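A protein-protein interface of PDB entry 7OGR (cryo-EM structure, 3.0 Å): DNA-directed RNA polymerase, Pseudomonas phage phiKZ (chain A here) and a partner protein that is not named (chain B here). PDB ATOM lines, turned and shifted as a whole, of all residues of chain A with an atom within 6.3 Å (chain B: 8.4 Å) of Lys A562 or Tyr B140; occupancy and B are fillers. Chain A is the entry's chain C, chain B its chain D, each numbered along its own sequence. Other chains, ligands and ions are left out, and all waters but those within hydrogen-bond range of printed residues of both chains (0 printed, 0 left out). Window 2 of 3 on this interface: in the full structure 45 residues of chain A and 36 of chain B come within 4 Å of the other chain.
The backbone NH (N) of Ala B142 sits at hydrogen-bond distance from the side-chain hydroxyl (OG) of Ser A176, 2.6 Å away. The backbone carbonyl oxygen (O) of Glu B139 lies within hydrogen-bond range of the backbone NH (N) of Lys A562 (2.8 Å).
Printed residues of chain A that touch a printed residue of chain B: Ser A176, Thr A560, Thr A561, Lys A562, Asp A563 and Asn A564. Of the 13 printed residues of chain B, 5 touch a printed residue of chain A. Hydrophobic or aromatic side chains of chain B that line the printed part of chain A: Tyr B140, Leu B141 and Ala B142. Among the printed residues, 9 pairs touch across the chains.
The side-chain amino group (NZ) of Lys A548 sits at hydrogen-bond distance from the backbone carbonyl oxygen (O) of Lys A562, at 2.4 Å. N of Thr A561 is in hydrogen-bond range of O of Val A549 (3.1 Å). The side-chain amino group (NZ) of Lys A562 is in salt-bridge range of the side-chain carboxylate (OD2) of Asp A563 (3.5 Å). The guanidinium group (NH2) of Arg B42 lies within hydrogen-bond range of the side-chain hydroxyl (OH) of Tyr B140, at 3.0 Å.
Lys A562 touches just these residues of chain B: Glu B139 (2.8 Å) and Tyr B140 (3.6 Å). Printed residues of chain A within 4 Å of Tyr B140: Lys A562 (3.6 Å). Of the printed residues of chain B, Ser A176 touches Leu B141 (3.3 Å) and Ala B142 (2.6 Å). Of the printed residues of chain B, Asp A563 touches Leu B141 and Thr B143. Printed residues of chain A within 4 Å of Thr B143: Asp A563 and Asn A564. Ser B138 touches none of the printed residues of chain A. Lys B136 touches none of the printed residues of chain A. The nearest printed residue of chain B that does not touch Thr A561 is Ser B138 (4.3 Å).
Ser A176 touches Leu B141. Glu B139 touches Thr A560. Glu B139 touches Thr A561. CE of Lys A562 touches CD1 of Tyr B140 (3.6 Å). Asp A563 touches Leu B141 (OD1 to O, 3.5 Å). Thr B143 touches Asp A563. CG2 of Thr B143 touches O of Asn A564, 3.7 Å away.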
ATOM      1  N   SER A 176     -26.808 -20.200  19.352  1.00  0.00           N
ATOM      2  CA  SER A 176     -25.719 -20.640  18.487  1.00  0.00           C
ATOM      3  C   SER A 176     -24.802 -21.616  19.215  1.00  0.00           C
ATOM      4  O   SER A 176     -23.577 -21.538  19.113  1.00  0.00           O
ATOM      5  CB  SER A 176     -24.926 -19.447  17.960  1.00  0.00           C
ATOM      6  OG  SER A 176     -24.480 -18.621  19.017  1.00  0.00           O
ATOM      7  N   LYS A 548     -32.537 -12.335  29.409  1.00  0.00           N
ATOM      8  CA  LYS A 548     -31.411 -13.246  29.299  1.00  0.00           C
ATOM      9  C   LYS A 548     -31.805 -14.654  29.731  1.00  0.00           C
ATOM     10  O   LYS A 548     -32.798 -14.865  30.430  1.00  0.00           O
ATOM     11  CB  LYS A 548     -30.230 -12.741  30.127  1.00  0.00           C
ATOM     12  CG  LYS A 548     -29.815 -11.327  29.766  1.00  0.00           C
ATOM     13  CD  LYS A 548     -28.574 -10.889  30.516  1.00  0.00           C
ATOM     14  CE  LYS A 548     -28.237  -9.444  30.199  1.00  0.00           C
ATOM     15  NZ  LYS A 548     -28.025  -9.236  28.739  1.00  0.00           N
ATOM     16  N   VAL A 549     -31.002 -15.624  29.299  1.00  0.00           N
ATOM     17  CA  VAL A 549     -31.322 -17.039  29.427  1.00  0.00           C
ATOM     18  C   VAL A 549     -30.147 -17.749  30.088  1.00  0.00           C
ATOM     19  O   VAL A 549     -29.010 -17.645  29.617  1.00  0.00           O
ATOM     20  CB  VAL A 549     -31.637 -17.667  28.054  1.00  0.00           C
ATOM     21  CG1 VAL A 549     -31.672 -19.169  28.146  1.00  0.00           C
ATOM     22  CG2 VAL A 549     -32.965 -17.153  27.524  1.00  0.00           C
ATOM     23  N   THR A 560     -25.014 -17.703  32.318  1.00  0.00           N
ATOM     24  CA  THR A 560     -26.089 -16.856  31.820  1.00  0.00           C
ATOM     25  C   THR A 560     -25.580 -16.101  30.602  1.00  0.00           C
ATOM     26  O   THR A 560     -24.502 -15.497  30.651  1.00  0.00           O
ATOM     27  CB  THR A 560     -26.567 -15.877  32.899  1.00  0.00           C
ATOM     28  OG1 THR A 560     -26.944 -16.606  34.073  1.00  0.00           O
ATOM     29  CG2 THR A 560     -27.761 -15.072  32.408  1.00  0.00           C
ATOM     30  N   THR A 561     -26.350 -16.139  29.516  1.00  0.00           N
ATOM     31  CA  THR A 561     -25.920 -15.549  28.257  1.00  0.00           C
ATOM     32  C   THR A 561     -25.929 -14.024  28.329  1.00  0.00           C
ATOM     33  O   THR A 561     -26.602 -13.411  29.163  1.00  0.00           O
ATOM     34  CB  THR A 561     -26.814 -16.019  27.109  1.00  0.00           C
ATOM     35  OG1 THR A 561     -28.175 -15.666  27.386  1.00  0.00           O
ATOM     36  CG2 THR A 561     -26.712 -17.526  26.937  1.00  0.00           C
ATOM     37  N   LYS A 562     -25.156 -13.412  27.430  1.00  0.00           N
ATOM     38  CA  LYS A 562     -25.053 -11.957  27.383  1.00  0.00           C
ATOM     39  C   LYS A 562     -26.214 -11.344  26.608  1.00  0.00           C
ATOM     40  O   LYS A 562     -26.695 -10.260  26.957  1.00  0.00           O
ATOM     41  CB  LYS A 562     -23.710 -11.557  26.761  1.00  0.00           C
ATOM     42  CG  LYS A 562     -23.398 -10.060  26.760  1.00  0.00           C
ATOM     43  CD  LYS A 562     -23.582  -9.432  25.379  1.00  0.00           C
ATOM     44  CE  LYS A 562     -22.529  -9.920  24.399  1.00  0.00           C
ATOM     45  NZ  LYS A 562     -22.709  -9.316  23.048  1.00  0.00           N
ATOM     46  N   ASP A 563     -26.683 -12.027  25.570  1.00  0.00           N
ATOM     47  CA  ASP A 563     -27.706 -11.493  24.686  1.00  0.00           C
ATOM     48  C   ASP A 563     -29.095 -11.697  25.276  1.00  0.00           C
ATOM     49  O   ASP A 563     -29.347 -12.655  26.010  1.00  0.00           O
ATOM     50  CB  ASP A 563     -27.630 -12.164  23.313  1.00  0.00           C
ATOM     51  CG  ASP A 563     -26.644 -11.485  22.383  1.00  0.00           C
ATOM     52  OD1 ASP A 563     -26.599 -11.858  21.192  1.00  0.00           O
ATOM     53  OD2 ASP A 563     -25.917 -10.580  22.840  1.00  0.00           O
ATOM     54  N   ASN A 564     -29.998 -10.775  24.950  1.00  0.00           N
ATOM     55  CA  ASN A 564     -31.406 -10.953  25.275  1.00  0.00           C
ATOM     56  C   ASN A 564     -32.020 -11.940  24.290  1.00  0.00           C
ATOM     57  O   ASN A 564     -32.050 -11.684  23.082  1.00  0.00           O
ATOM     58  CB  ASN A 564     -32.137  -9.615  25.229  1.00  0.00           C
ATOM     59  CG  ASN A 564     -31.847  -8.752  26.438  1.00  0.00           C
ATOM     60  OD1 ASN A 564     -31.319  -9.228  27.441  1.00  0.00           O
ATOM     61  ND2 ASN A 564     -32.193  -7.473  26.349  1.00  0.00           N
ATOM     62  N   TRP B  20      -6.373 -16.766  28.915  1.00  0.00           N
ATOM     63  CA  TRP B  20      -7.766 -16.333  28.927  1.00  0.00           C
ATOM     64  C   TRP B  20      -8.044 -15.344  30.054  1.00  0.00           C
ATOM     65  O   TRP B  20      -8.950 -14.514  29.933  1.00  0.00           O
ATOM     66  CB  TRP B  20      -8.694 -17.543  29.031  1.00  0.00           C
ATOM     67  CG  TRP B  20      -8.893 -18.262  27.729  1.00  0.00           C
ATOM     68  CD1 TRP B  20      -8.279 -19.411  27.324  1.00  0.00           C
ATOM     69  CD2 TRP B  20      -9.765 -17.875  26.658  1.00  0.00           C
ATOM     70  NE1 TRP B  20      -8.715 -19.766  26.071  1.00  0.00           N
ATOM     71  CE2 TRP B  20      -9.628 -18.840  25.639  1.00  0.00           C
ATOM     72  CE3 TRP B  20     -10.649 -16.809  26.462  1.00  0.00           C
ATOM     73  CZ2 TRP B  20     -10.341 -18.770  24.444  1.00  0.00           C
ATOM     74  CZ3 TRP B  20     -11.356 -16.742  25.274  1.00  0.00           C
ATOM     75  CH2 TRP B  20     -11.198 -17.716  24.281  1.00  0.00           C
ATOM     76  N   ARG B  42      -9.298  -9.202  23.234  1.00  0.00           N
ATOM     77  CA  ARG B  42     -10.135 -10.239  22.639  1.00  0.00           C
ATOM     78  C   ARG B  42      -9.683 -10.622  21.237  1.00  0.00           C
ATOM     79  O   ARG B  42     -10.070 -11.687  20.744  1.00  0.00           O
ATOM     80  CB  ARG B  42     -11.594  -9.785  22.610  1.00  0.00           C
ATOM     81  CG  ARG B  42     -12.223  -9.647  23.985  1.00  0.00           C
ATOM     82  CD  ARG B  42     -13.713  -9.373  23.882  1.00  0.00           C
ATOM     83  NE  ARG B  42     -14.343  -9.267  25.194  1.00  0.00           N
ATOM     84  CZ  ARG B  42     -15.642  -9.059  25.381  1.00  0.00           C
ATOM     85  NH1 ARG B  42     -16.452  -8.936  24.339  1.00  0.00           N
ATOM     86  NH2 ARG B  42     -16.133  -8.975  26.610  1.00  0.00           N
ATOM     87  N   THR B 133     -12.506 -22.282  22.294  1.00  0.00           N
ATOM     88  CA  THR B 133     -13.532 -21.287  22.012  1.00  0.00           C
ATOM     89  C   THR B 133     -14.944 -21.763  22.331  1.00  0.00           C
ATOM     90  O   THR B 133     -15.808 -20.925  22.598  1.00  0.00           O
ATOM     91  CB  THR B 133     -13.455 -20.845  20.549  1.00  0.00           C
ATOM     92  OG1 THR B 133     -13.293 -21.992  19.705  1.00  0.00           O
ATOM     93  CG2 THR B 133     -12.294 -19.886  20.345  1.00  0.00           C
ATOM     94  N   THR B 134     -15.215 -23.072  22.309  1.00  0.00           N
ATOM     95  CA  THR B 134     -16.553 -23.508  22.711  1.00  0.00           C
ATOM     96  C   THR B 134     -16.716 -23.513  24.226  1.00  0.00           C
ATOM     97  O   THR B 134     -17.798 -23.199  24.736  1.00  0.00           O
ATOM     98  CB  THR B 134     -16.878 -24.883  22.132  1.00  0.00           C
ATOM     99  OG1 THR B 134     -15.995 -25.870  22.686  1.00  0.00           O
ATOM    100  CG2 THR B 134     -16.796 -24.859  20.622  1.00  0.00           C
ATOM    101  N   LYS B 136     -14.748 -21.750  26.638  1.00  0.00           N
ATOM    102  CA  LYS B 136     -14.551 -20.469  27.307  1.00  0.00           C
ATOM    103  C   LYS B 136     -15.600 -19.438  26.911  1.00  0.00           C
ATOM    104  O   LYS B 136     -15.868 -18.512  27.686  1.00  0.00           O
ATOM    105  CB  LYS B 136     -13.148 -19.937  27.020  1.00  0.00           C
ATOM    106  CG  LYS B 136     -12.095 -20.457  27.985  1.00  0.00           C
ATOM    107  CD  LYS B 136     -12.446 -20.100  29.422  1.00  0.00           C
ATOM    108  CE  LYS B 136     -11.207 -20.022  30.297  1.00  0.00           C
ATOM    109  NZ  LYS B 136     -10.317 -21.200  30.103  1.00  0.00           N
ATOM    110  N   LEU B 137     -16.203 -19.573  25.735  1.00  0.00           N
ATOM    111  CA  LEU B 137     -17.245 -18.658  25.272  1.00  0.00           C
ATOM    112  C   LEU B 137     -18.576 -19.406  25.301  1.00  0.00           C
ATOM    113  O   LEU B 137     -18.995 -20.000  24.306  1.00  0.00           O
ATOM    114  CB  LEU B 137     -16.933 -18.130  23.879  1.00  0.00           C
ATOM    115  CG  LEU B 137     -15.579 -17.439  23.718  1.00  0.00           C
ATOM    116  CD1 LEU B 137     -15.382 -17.002  22.278  1.00  0.00           C
ATOM    117  CD2 LEU B 137     -15.452 -16.262  24.671  1.00  0.00           C
ATOM    118  N   SER B 138     -19.239 -19.372  26.456  1.00  0.00           N
ATOM    119  CA  SER B 138     -20.548 -19.986  26.616  1.00  0.00           C
ATOM    120  C   SER B 138     -21.660 -18.976  26.847  1.00  0.00           C
ATOM    121  O   SER B 138     -22.834 -19.336  26.710  1.00  0.00           O
ATOM    122  CB  SER B 138     -20.532 -20.991  27.778  1.00  0.00           C
ATOM    123  OG  SER B 138     -19.651 -22.068  27.508  1.00  0.00           O
ATOM    124  N   GLU B 139     -21.329 -17.732  27.192  1.00  0.00           N
ATOM    125  CA  GLU B 139     -22.311 -16.672  27.353  1.00  0.00           C
ATOM    126  C   GLU B 139     -22.450 -15.802  26.113  1.00  0.00           C
ATOM    127  O   GLU B 139     -23.405 -15.022  26.024  1.00  0.00           O
ATOM    128  CB  GLU B 139     -21.943 -15.793  28.554  1.00  0.00           C
ATOM    129  CG  GLU B 139     -21.265 -16.554  29.681  1.00  0.00           C
ATOM    130  CD  GLU B 139     -21.038 -15.698  30.912  1.00  0.00           C
ATOM    131  OE1 GLU B 139     -20.876 -14.468  30.762  1.00  0.00           O
ATOM    132  OE2 GLU B 139     -21.019 -16.256  32.029  1.00  0.00           O
ATOM    133  N   TYR B 140     -21.523 -15.913  25.160  1.00  0.00           N
ATOM    134  CA  TYR B 140     -21.565 -15.134  23.925  1.00  0.00           C
ATOM    135  C   TYR B 140     -22.159 -16.015  22.831  1.00  0.00           C
ATOM    136  O   TYR B 140     -21.462 -16.544  21.966  1.00  0.00           O
ATOM    137  CB  TYR B 140     -20.170 -14.633  23.562  1.00  0.00           C
ATOM    138  CG  TYR B 140     -19.553 -13.732  24.608  1.00  0.00           C
ATOM    139  CD1 TYR B 140     -19.835 -12.371  24.633  1.00  0.00           C
ATOM    140  CD2 TYR B 140     -18.693 -14.244  25.572  1.00  0.00           C
ATOM    141  CE1 TYR B 140     -19.275 -11.544  25.590  1.00  0.00           C
ATOM    142  CE2 TYR B 140     -18.129 -13.425  26.533  1.00  0.00           C
ATOM    143  CZ  TYR B 140     -18.424 -12.077  26.537  1.00  0.00           C
ATOM    144  OH  TYR B 140     -17.864 -11.258  27.490  1.00  0.00           O
ATOM    145  N   LEU B 141     -23.478 -16.171  22.880  1.00  0.00           N
ATOM    146  CA  LEU B 141     -24.215 -16.986  21.925  1.00  0.00           C
ATOM    147  C   LEU B 141     -25.085 -16.087  21.059  1.00  0.00           C
ATOM    148  O   LEU B 141     -25.880 -15.297  21.580  1.00  0.00           O
ATOM    149  CB  LEU B 141     -25.077 -18.030  22.640  1.00  0.00           C
ATOM    150  CG  LEU B 141     -24.352 -19.212  23.290  1.00  0.00           C
ATOM    151  CD1 LEU B 141     -25.351 -20.257  23.759  1.00  0.00           C
ATOM    152  CD2 LEU B 141     -23.346 -19.831  22.331  1.00  0.00           C
ATOM    153  N   ALA B 142     -24.932 -16.208  19.742  1.00  0.00           N
ATOM    154  CA  ALA B 142     -25.702 -15.395  18.811  1.00  0.00           C
ATOM    155  C   ALA B 142     -27.136 -15.907  18.736  1.00  0.00           C
ATOM    156  O   ALA B 142     -27.369 -17.082  18.435  1.00  0.00           O
ATOM    157  CB  ALA B 142     -25.052 -15.413  17.431  1.00  0.00           C
ATOM    158  N   THR B 143     -28.092 -15.027  19.011  1.00  0.00           N
ATOM    159  CA  THR B 143     -29.505 -15.371  19.009  1.00  0.00           C
ATOM    160  C   THR B 143     -30.224 -14.676  17.860  1.00  0.00           C
ATOM    161  O   THR B 143     -29.718 -13.727  17.257  1.00  0.00           O
ATOM    162  CB  THR B 143     -30.167 -14.989  20.338  1.00  0.00           C
ATOM    163  OG1 THR B 143     -31.556 -15.335  20.295  1.00  0.00           O
ATOM    164  CG2 THR B 143     -30.028 -13.496  20.596  1.00  0.00           C
ATOM    165  N   GLY B 192     -24.225  -4.771  16.528  1.00  0.00           N
ATOM    166  CA  GLY B 192     -24.739  -5.817  17.385  1.00  0.00           C
ATOM    167  C   GLY B 192     -25.857  -6.654  16.802  1.00  0.00           C
ATOM    168  O   GLY B 192     -26.362  -7.546  17.495  1.00  0.00           O
